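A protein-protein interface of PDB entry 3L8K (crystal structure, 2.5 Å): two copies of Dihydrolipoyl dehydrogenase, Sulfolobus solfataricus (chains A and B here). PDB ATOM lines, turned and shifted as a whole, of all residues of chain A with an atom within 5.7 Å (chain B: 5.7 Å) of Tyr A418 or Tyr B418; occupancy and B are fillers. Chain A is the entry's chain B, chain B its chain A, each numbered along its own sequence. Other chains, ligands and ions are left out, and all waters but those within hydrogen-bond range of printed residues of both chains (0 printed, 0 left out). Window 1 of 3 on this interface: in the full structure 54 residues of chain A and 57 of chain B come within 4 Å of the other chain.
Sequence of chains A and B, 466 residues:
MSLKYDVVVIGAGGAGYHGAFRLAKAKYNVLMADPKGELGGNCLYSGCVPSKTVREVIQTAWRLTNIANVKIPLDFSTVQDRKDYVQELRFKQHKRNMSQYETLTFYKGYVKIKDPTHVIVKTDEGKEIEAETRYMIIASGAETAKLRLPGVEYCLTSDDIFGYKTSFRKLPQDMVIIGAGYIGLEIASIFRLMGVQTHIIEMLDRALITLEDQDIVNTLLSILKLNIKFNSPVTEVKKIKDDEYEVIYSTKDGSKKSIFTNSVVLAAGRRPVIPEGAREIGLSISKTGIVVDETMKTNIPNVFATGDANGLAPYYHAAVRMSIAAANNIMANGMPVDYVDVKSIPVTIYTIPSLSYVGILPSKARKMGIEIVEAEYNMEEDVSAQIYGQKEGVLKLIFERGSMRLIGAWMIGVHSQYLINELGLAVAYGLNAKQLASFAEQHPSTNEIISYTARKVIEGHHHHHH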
ATOM      1  N   SER A 384       1.886  21.268 -10.899  1.00  0.00           N
ATOM      2  CA  SER A 384       1.034  21.048  -9.729  1.00  0.00           C
ATOM      3  C   SER A 384       0.499  19.637  -9.681  1.00  0.00           C
ATOM      4  O   SER A 384       0.342  19.074  -8.600  1.00  0.00           O
ATOM      5  CB  SER A 384      -0.093  22.061  -9.675  1.00  0.00           C
ATOM      6  OG  SER A 384       0.463  23.371  -9.516  1.00  0.00           O
ATOM      7  N   HIS A 415      -7.291  21.518 -10.841  1.00  0.00           N
ATOM      8  CA  HIS A 415      -7.517  22.900 -11.130  1.00  0.00           C
ATOM      9  C   HIS A 415      -8.265  23.116 -12.424  1.00  0.00           C
ATOM     10  O   HIS A 415      -8.239  24.227 -12.961  1.00  0.00           O
ATOM     11  CB  HIS A 415      -6.231  23.679 -11.145  1.00  0.00           C
ATOM     12  CG  HIS A 415      -5.452  23.558  -9.885  1.00  0.00           C
ATOM     13  ND1 HIS A 415      -6.047  23.278  -8.670  1.00  0.00           N
ATOM     14  CD2 HIS A 415      -4.123  23.709  -9.638  1.00  0.00           C
ATOM     15  CE1 HIS A 415      -5.108  23.250  -7.735  1.00  0.00           C
ATOM     16  NE2 HIS A 415      -3.936  23.501  -8.295  1.00  0.00           N
ATOM     17  N   SER A 416      -8.949  22.099 -12.930  1.00  0.00           N
ATOM     18  CA  SER A 416      -9.751  22.324 -14.102  1.00  0.00           C
ATOM     19  C   SER A 416     -10.732  23.464 -13.813  1.00  0.00           C
ATOM     20  O   SER A 416     -11.034  24.226 -14.703  1.00  0.00           O
ATOM     21  CB  SER A 416     -10.480  21.056 -14.560  1.00  0.00           C
ATOM     22  OG  SER A 416     -11.615  20.734 -13.784  1.00  0.00           O
ATOM     23  N   GLN A 417     -11.191  23.605 -12.559  1.00  0.00           N
ATOM     24  CA  GLN A 417     -12.161  24.646 -12.242  1.00  0.00           C
ATOM     25  C   GLN A 417     -11.599  26.057 -12.392  1.00  0.00           C
ATOM     26  O   GLN A 417     -12.389  26.950 -12.534  1.00  0.00           O
ATOM     27  CB  GLN A 417     -12.799  24.489 -10.838  1.00  0.00           C
ATOM     28  CG  GLN A 417     -11.920  24.907  -9.747  1.00  0.00           C
ATOM     29  CD  GLN A 417     -12.507  24.645  -8.373  1.00  0.00           C
ATOM     30  OE1 GLN A 417     -13.594  25.136  -8.021  1.00  0.00           O
ATOM     31  NE2 GLN A 417     -11.771  23.897  -7.574  1.00  0.00           N
ATOM     32  N   TYR A 418     -10.279  26.249 -12.316  1.00  0.00           N
ATOM     33  CA  TYR A 418      -9.673  27.562 -12.499  1.00  0.00           C
ATOM     34  C   TYR A 418      -9.338  27.762 -13.939  1.00  0.00           C
ATOM     35  O   TYR A 418      -9.694  28.764 -14.510  1.00  0.00           O
ATOM     36  CB  TYR A 418      -8.415  27.776 -11.632  1.00  0.00           C
ATOM     37  CG  TYR A 418      -8.718  27.539 -10.188  1.00  0.00           C
ATOM     38  CD1 TYR A 418      -9.375  28.479  -9.431  1.00  0.00           C
ATOM     39  CD2 TYR A 418      -8.432  26.337  -9.612  1.00  0.00           C
ATOM     40  CE1 TYR A 418      -9.712  28.220  -8.124  1.00  0.00           C
ATOM     41  CE2 TYR A 418      -8.746  26.074  -8.338  1.00  0.00           C
ATOM     42  CZ  TYR A 418      -9.385  27.012  -7.588  1.00  0.00           C
ATOM     43  OH  TYR A 418      -9.675  26.696  -6.284  1.00  0.00           O
ATOM     44  N   LEU A 419      -8.675  26.801 -14.542  1.00  0.00           N
ATOM     45  CA  LEU A 419      -8.333  26.891 -15.953  1.00  0.00           C
ATOM     46  C   LEU A 419      -9.513  27.186 -16.883  1.00  0.00           C
ATOM     47  O   LEU A 419      -9.391  27.987 -17.815  1.00  0.00           O
ATOM     48  CB  LEU A 419      -7.619  25.616 -16.429  1.00  0.00           C
ATOM     49  CG  LEU A 419      -6.109  25.745 -16.293  1.00  0.00           C
ATOM     50  CD1 LEU A 419      -5.678  26.034 -14.820  1.00  0.00           C
ATOM     51  CD2 LEU A 419      -5.419  24.503 -16.849  1.00  0.00           C
ATOM     52  N   ILE A 420     -10.640  26.532 -16.646  1.00  0.00           N
ATOM     53  CA  ILE A 420     -11.821  26.716 -17.483  1.00  0.00           C
ATOM     54  C   ILE A 420     -12.349  28.139 -17.573  1.00  0.00           C
ATOM     55  O   ILE A 420     -12.999  28.471 -18.533  1.00  0.00           O
ATOM     56  CB  ILE A 420     -12.974  25.797 -17.050  1.00  0.00           C
ATOM     57  CG1 ILE A 420     -13.819  25.456 -18.272  1.00  0.00           C
ATOM     58  CG2 ILE A 420     -13.787  26.420 -15.878  1.00  0.00           C
ATOM     59  CD1 ILE A 420     -13.128  24.490 -19.240  1.00  0.00           C
ATOM     60  N   ASN A 421     -12.066  28.979 -16.600  1.00  0.00           N
ATOM     61  CA  ASN A 421     -12.501  30.367 -16.645  1.00  0.00           C
ATOM     62  C   ASN A 421     -11.676  31.177 -17.594  1.00  0.00           C
ATOM     63  O   ASN A 421     -12.228  31.982 -18.345  1.00  0.00           O
ATOM     64  CB  ASN A 421     -12.439  30.987 -15.273  1.00  0.00           C
ATOM     65  CG  ASN A 421     -13.313  30.258 -14.293  1.00  0.00           C
ATOM     66  OD1 ASN A 421     -14.484  29.999 -14.581  1.00  0.00           O
ATOM     67  ND2 ASN A 421     -12.755  29.905 -13.140  1.00  0.00           N
ATOM     68  N   GLU A 422     -10.362  30.981 -17.577  1.00  0.00           N
ATOM     69  CA  GLU A 422      -9.494  31.616 -18.586  1.00  0.00           C
ATOM     70  C   GLU A 422      -9.988  31.217 -19.983  1.00  0.00           C
ATOM     71  O   GLU A 422     -10.212  32.054 -20.879  1.00  0.00           O
ATOM     72  CB  GLU A 422      -8.012  31.186 -18.382  1.00  0.00           C
ATOM     73  CG  GLU A 422      -6.987  32.078 -19.060  1.00  0.00           C
ATOM     74  CD  GLU A 422      -5.586  31.397 -19.288  1.00  0.00           C
ATOM     75  OE1 GLU A 422      -5.003  30.812 -18.307  1.00  0.00           O
ATOM     76  OE2 GLU A 422      -5.076  31.467 -20.459  1.00  0.00           O
ATOM     77  N   SER A 445       1.923  28.186 -12.337  1.00  0.00           N
ATOM     78  CA  SER A 445       0.486  27.828 -12.181  1.00  0.00           C
ATOM     79  C   SER A 445       0.091  26.801 -13.225  1.00  0.00           C
ATOM     80  O   SER A 445       0.707  26.710 -14.269  1.00  0.00           O
ATOM     81  CB  SER A 445      -0.435  29.046 -12.297  1.00  0.00           C
ATOM     82  OG  SER A 445      -0.548  29.499 -13.643  1.00  0.00           O
ATOM     83  N   THR A 446      -0.951  26.034 -12.966  1.00  0.00           N
ATOM     84  CA  THR A 446      -1.393  25.048 -13.960  1.00  0.00           C
ATOM     85  C   THR A 446      -1.881  25.712 -15.271  1.00  0.00           C
ATOM     86  O   THR A 446      -1.884  25.077 -16.339  1.00  0.00           O
ATOM     87  CB  THR A 446      -2.455  24.100 -13.375  1.00  0.00           C
ATOM     88  OG1 THR A 446      -1.966  23.504 -12.166  1.00  0.00           O
ATOM     89  CG2 THR A 446      -2.748  22.993 -14.339  1.00  0.00           C
ATOM     90  N   ASN A 447      -2.235  27.002 -15.193  1.00  0.00           N
ATOM     91  CA  ASN A 447      -2.615  27.798 -16.385  1.00  0.00           C
ATOM     92  C   ASN A 447      -1.582  27.839 -17.502  1.00  0.00           C
ATOM     93  O   ASN A 447      -1.956  28.070 -18.623  1.00  0.00           O
ATOM     94  CB  ASN A 447      -2.968  29.249 -16.018  1.00  0.00           C
ATOM     95  CG  ASN A 447      -4.229  29.363 -15.207  1.00  0.00           C
ATOM     96  OD1 ASN A 447      -4.229  29.106 -13.997  1.00  0.00           O
ATOM     97  ND2 ASN A 447      -5.318  29.779 -15.861  1.00  0.00           N
ATOM     98  N   GLU B  56       3.840  24.818  -1.597  1.00  0.00           N
ATOM     99  CA  GLU B  56       2.588  24.035  -1.611  1.00  0.00           C
ATOM    100  C   GLU B  56       2.515  23.038  -0.482  1.00  0.00           C
ATOM    101  O   GLU B  56       1.452  22.887   0.103  1.00  0.00           O
ATOM    102  CB  GLU B  56       2.361  23.231  -2.884  1.00  0.00           C
ATOM    103  CG  GLU B  56       1.826  23.990  -4.029  1.00  0.00           C
ATOM    104  CD  GLU B  56       0.464  24.606  -3.768  1.00  0.00           C
ATOM    105  OE1 GLU B  56      -0.421  23.910  -3.193  1.00  0.00           O
ATOM    106  OE2 GLU B  56       0.291  25.793  -4.149  1.00  0.00           O
ATOM    107  N   SER B 384     -13.599  29.809  -1.051  1.00  0.00           N
ATOM    108  CA  SER B 384     -12.353  29.069  -0.772  1.00  0.00           C
ATOM    109  C   SER B 384     -11.538  29.732   0.339  1.00  0.00           C
ATOM    110  O   SER B 384     -10.980  29.057   1.209  1.00  0.00           O
ATOM    111  CB  SER B 384     -11.481  29.013  -2.028  1.00  0.00           C
ATOM    112  OG  SER B 384     -12.117  28.298  -3.066  1.00  0.00           O
ATOM    113  N   TYR B 388     -10.722  27.501   3.835  1.00  0.00           N
ATOM    114  CA  TYR B 388      -9.363  27.335   4.307  1.00  0.00           C
ATOM    115  C   TYR B 388      -8.968  28.245   5.455  1.00  0.00           C
ATOM    116  O   TYR B 388      -7.868  28.117   5.961  1.00  0.00           O
ATOM    117  CB  TYR B 388      -8.385  27.632   3.196  1.00  0.00           C
ATOM    118  CG  TYR B 388      -8.419  26.773   1.982  1.00  0.00           C
ATOM    119  CD1 TYR B 388      -8.644  25.400   2.054  1.00  0.00           C
ATOM    120  CD2 TYR B 388      -8.106  27.338   0.740  1.00  0.00           C
ATOM    121  CE1 TYR B 388      -8.608  24.608   0.888  1.00  0.00           C
ATOM    122  CE2 TYR B 388      -8.058  26.580  -0.413  1.00  0.00           C
ATOM    123  CZ  TYR B 388      -8.306  25.219  -0.348  1.00  0.00           C
ATOM    124  OH  TYR B 388      -8.253  24.508  -1.533  1.00  0.00           O
ATOM    125  N   HIS B 415      -5.225  31.919  -4.196  1.00  0.00           N
ATOM    126  CA  HIS B 415      -5.381  31.662  -5.618  1.00  0.00           C
ATOM    127  C   HIS B 415      -5.105  32.846  -6.539  1.00  0.00           C
ATOM    128  O   HIS B 415      -5.540  32.814  -7.690  1.00  0.00           O
ATOM    129  CB  HIS B 415      -6.765  31.066  -5.941  1.00  0.00           C
ATOM    130  CG  HIS B 415      -7.088  29.789  -5.223  1.00  0.00           C
ATOM    131  ND1 HIS B 415      -6.160  28.791  -4.994  1.00  0.00           N
ATOM    132  CD2 HIS B 415      -8.252  29.344  -4.690  1.00  0.00           C
ATOM    133  CE1 HIS B 415      -6.746  27.788  -4.355  1.00  0.00           C
ATOM    134  NE2 HIS B 415      -8.012  28.103  -4.151  1.00  0.00           N
ATOM    135  N   SER B 416      -4.390  33.877  -6.084  1.00  0.00           N
ATOM    136  CA  SER B 416      -4.119  35.016  -6.956  1.00  0.00           C
ATOM    137  C   SER B 416      -3.317  34.579  -8.191  1.00  0.00           C
ATOM    138  O   SER B 416      -3.476  35.120  -9.250  1.00  0.00           O
ATOM    139  CB  SER B 416      -3.353  36.113  -6.237  1.00  0.00           C
ATOM    140  OG  SER B 416      -2.029  35.716  -5.937  1.00  0.00           O
ATOM    141  N   GLN B 417      -2.472  33.583  -8.065  1.00  0.00           N
ATOM    142  CA  GLN B 417      -1.753  33.117  -9.217  1.00  0.00           C
ATOM    143  C   GLN B 417      -2.671  32.582 -10.318  1.00  0.00           C
ATOM    144  O   GLN B 417      -2.258  32.572 -11.459  1.00  0.00           O
ATOM    145  CB  GLN B 417      -0.756  32.030  -8.849  1.00  0.00           C
ATOM    146  CG  GLN B 417      -1.353  30.731  -8.379  1.00  0.00           C
ATOM    147  CD  GLN B 417      -0.278  29.685  -8.093  1.00  0.00           C
ATOM    148  OE1 GLN B 417       0.830  29.696  -8.697  1.00  0.00           O
ATOM    149  NE2 GLN B 417      -0.597  28.752  -7.191  1.00  0.00           N
ATOM    150  N   TYR B 418      -3.881  32.103  -9.992  1.00  0.00           N
ATOM    151  CA  TYR B 418      -4.763  31.554 -11.040  1.00  0.00           C
ATOM    152  C   TYR B 418      -5.586  32.663 -11.599  1.00  0.00           C
ATOM    153  O   TYR B 418      -5.715  32.809 -12.803  1.00  0.00           O
ATOM    154  CB  TYR B 418      -5.667  30.435 -10.522  1.00  0.00           C
ATOM    155  CG  TYR B 418      -4.861  29.348  -9.889  1.00  0.00           C
ATOM    156  CD1 TYR B 418      -4.157  28.421 -10.664  1.00  0.00           C
ATOM    157  CD2 TYR B 418      -4.727  29.283  -8.522  1.00  0.00           C
ATOM    158  CE1 TYR B 418      -3.351  27.427 -10.062  1.00  0.00           C
ATOM    159  CE2 TYR B 418      -3.944  28.302  -7.917  1.00  0.00           C
ATOM    160  CZ  TYR B 418      -3.260  27.387  -8.699  1.00  0.00           C
ATOM    161  OH  TYR B 418      -2.499  26.455  -8.060  1.00  0.00           O
ATOM    162  N   LEU B 419      -6.140  33.468 -10.712  1.00  0.00           N
ATOM    163  CA  LEU B 419      -6.946  34.601 -11.130  1.00  0.00           C
ATOM    164  C   LEU B 419      -6.190  35.601 -11.987  1.00  0.00           C
ATOM    165  O   LEU B 419      -6.758  36.128 -12.910  1.00  0.00           O
ATOM    166  CB  LEU B 419      -7.504  35.294  -9.917  1.00  0.00           C
ATOM    167  CG  LEU B 419      -8.831  34.717  -9.446  1.00  0.00           C
ATOM    168  CD1 LEU B 419      -8.684  33.287  -8.984  1.00  0.00           C
ATOM    169  CD2 LEU B 419      -9.392  35.602  -8.368  1.00  0.00           C
ATOM    170  N   ILE B 420      -4.907  35.858 -11.680  1.00  0.00           N
ATOM    171  CA  ILE B 420      -4.125  36.825 -12.435  1.00  0.00           C
ATOM    172  C   ILE B 420      -4.039  36.511 -13.925  1.00  0.00           C
ATOM    173  O   ILE B 420      -3.837  37.431 -14.719  1.00  0.00           O
ATOM    174  CB  ILE B 420      -2.687  37.000 -11.883  1.00  0.00           C
ATOM    175  CG1 ILE B 420      -2.162  38.377 -12.300  1.00  0.00           C
ATOM    176  CG2 ILE B 420      -1.729  35.846 -12.310  1.00  0.00           C
ATOM    177  CD1 ILE B 420      -3.080  39.518 -11.822  1.00  0.00           C
ATOM    178  N   ASN B 421      -4.220  35.243 -14.308  1.00  0.00           N
ATOM    179  CA  ASN B 421      -4.096  34.831 -15.710  1.00  0.00           C
ATOM    180  C   ASN B 421      -5.339  35.154 -16.485  1.00  0.00           C
ATOM    181  O   ASN B 421      -5.272  35.612 -17.633  1.00  0.00           O
ATOM    182  CB  ASN B 421      -3.852  33.340 -15.843  1.00  0.00           C
ATOM    183  CG  ASN B 421      -2.597  32.923 -15.219  1.00  0.00           C
ATOM    184  OD1 ASN B 421      -1.583  33.545 -15.457  1.00  0.00           O
ATOM    185  ND2 ASN B 421      -2.639  31.887 -14.376  1.00  0.00           N
ATOM    186  N   GLU B 422      -6.479  34.878 -15.869  1.00  0.00           N
ATOM    187  CA  GLU B 422      -7.748  35.319 -16.432  1.00  0.00           C
ATOM    188  C   GLU B 422      -7.700  36.811 -16.664  1.00  0.00           C
ATOM    189  O   GLU B 422      -7.996  37.270 -17.711  1.00  0.00           O
ATOM    190  CB  GLU B 422      -8.913  34.950 -15.510  1.00  0.00           C
ATOM    191  CG  GLU B 422     -10.210  35.504 -15.971  1.00  0.00           C
ATOM    192  CD  GLU B 422     -11.423  35.040 -15.115  1.00  0.00           C
ATOM    193  OE1 GLU B 422     -11.227  34.104 -14.285  1.00  0.00           O
ATOM    194  OE2 GLU B 422     -12.552  35.620 -15.288  1.00  0.00           O
ATOM    195  N   SER B 445     -15.638  28.547  -7.610  1.00  0.00           N
ATOM    196  CA  SER B 445     -14.204  28.894  -7.672  1.00  0.00           C
ATOM    197  C   SER B 445     -13.978  30.367  -7.372  1.00  0.00           C
ATOM    198  O   SER B 445     -14.886  31.184  -7.482  1.00  0.00           O
ATOM    199  CB  SER B 445     -13.604  28.553  -9.035  1.00  0.00           C
ATOM    200  OG  SER B 445     -13.999  29.490 -10.025  1.00  0.00           O
ATOM    201  N   THR B 446     -12.755  30.696  -6.994  1.00  0.00           N
ATOM    202  CA  THR B 446     -12.400  32.042  -6.564  1.00  0.00           C
ATOM    203  C   THR B 446     -12.477  33.033  -7.739  1.00  0.00           C
ATOM    204  O   THR B 446     -12.761  34.203  -7.530  1.00  0.00           O
ATOM    205  CB  THR B 446     -11.001  32.043  -5.848  1.00  0.00           C
ATOM    206  OG1 THR B 446     -11.077  31.257  -4.652  1.00  0.00           O
ATOM    207  CG2 THR B 446     -10.546  33.465  -5.470  1.00  0.00           C
ATOM    208  N   ASN B 447     -12.278  32.555  -8.970  1.00  0.00           N
ATOM    209  CA  ASN B 447     -12.469  33.391 -10.162  1.00  0.00           C
ATOM    210  C   ASN B 447     -13.848  34.045 -10.218  1.00  0.00           C
ATOM    211  O   ASN B 447     -14.014  35.058 -10.911  1.00  0.00           O
ATOM    212  CB  ASN B 447     -12.285  32.597 -11.448  1.00  0.00           C
ATOM    213  CG  ASN B 447     -10.854  32.105 -11.652  1.00  0.00           C
ATOM    214  OD1 ASN B 447     -10.444  31.122 -11.054  1.00  0.00           O
ATOM    215  ND2 ASN B 447     -10.130  32.738 -12.547  1.00  0.00           N
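The side-chain hydroxyl (OH) of Tyr A418 is in hydrogen-bond range of a ring nitrogen (NE2) of His B415, 3.0 Å away. NE2 of His A415 is in hydrogen-bond range of OH of Tyr B418 (3.3 Å). ND2 of Asn B421 sits at hydrogen-bond distance from OG of Ser A445, at 3.3 Å. ND2 of Asn B421 sits close to OD1 of Asn A447, 3.2 Å away. The side-chain hydroxyl of Ser B445 sits at hydrogen-bond distance from the side-chain amide nitrogen of Asn A421 (3.4 Å). The side-chain amide oxygen (OD1) of Asn B447 lies close to the side-chain amide nitrogen (ND2) of Asn A421, at 3.3 Å.
NE2 of Gln B417 is in hydrogen-bond range of OH of Tyr B418, 3.1 Å away. O of Gln B417 lies within hydrogen-bond range of ND2 of Asn B421. The side-chain amide nitrogen of Asn B447 lies within hydrogen-bond range of the side-chain carboxylate of Glu B422. The backbone carbonyl oxygen (O) of Gln A417 lies within hydrogen-bond range of the side-chain amide nitrogen (ND2) of Asn A421, at 3.0 Å. ND2 of Asn A447 lies within hydrogen-bond range of OE1 of Glu A422 (2.7 Å). OG of Ser A445 sits close to N of Asn A447 (3.4 Å).
Among the printed residues, merely in contact across the chains: Gln A417 with Ser B445 (3.6 Å), Tyr A418 with Tyr B418 (3.98 Å), Tyr A418 with Asn B447 (3.3 Å), Asn A421 with Glu B422 (3.5 Å), Glu A422 with Asn B421 (3.7 Å), Ser A445 with Gln B417 (3.9 Å) and Asn A447 with Tyr B418 (3.4 Å).
Of the printed residues of chain B, Tyr A418 touches His B415 (3.0 Å), Tyr B418 (3.98 Å) and Asn B447 (3.3 Å). Printed residues of chain B within 4 Å of Asn A421: Glu B422 (3.5 Å), Ser B445 (3.4 Å) and Asn B447 (3.2 Å). Of the printed residues of chain A, Tyr B418 touches His A415, Tyr A418 and Asn A447. Of the printed residues of chain A, Glu B422 touches Asn A421 (3.5 Å). Of the printed residues of chain A, Ser B445 touches Gln A417 and Asn A421. Of the printed residues of chain A, Asn B447 touches Tyr A418 (3.3 Å) and Asn A421 (3.2 Å). The nearest printed residue of chain B that does not touch Tyr A418 is Ser B445 (4.01 Å). The nearest printed residue of chain A that does not touch Tyr B418 is Ser A445 (4.01 Å).
Of the 14 printed residues of chain B, 7 touch a printed residue of chain A. Of the 12 printed residues of chain A, 7 touch a printed residue of chain B. Hydrophobic or aromatic side chains of chain A within 4 Å of the printed part of chain B: His A415 and Tyr A418.
His A415 touches Tyr B418, and with the chains exchanged Tyr A418 touches His B415. Gln A417 touches Ser B445, and with the chains exchanged Ser A445 touches Gln B417. Tyr B418 touches its own counterpart, Tyr A418. Asn A421 touches Ser B445, and with the chains exchanged Ser A445 touches Asn B421. Of the 13 pairs that touch across the chains among the printed residues, 13 have their exchanged pair printed and touching as well.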
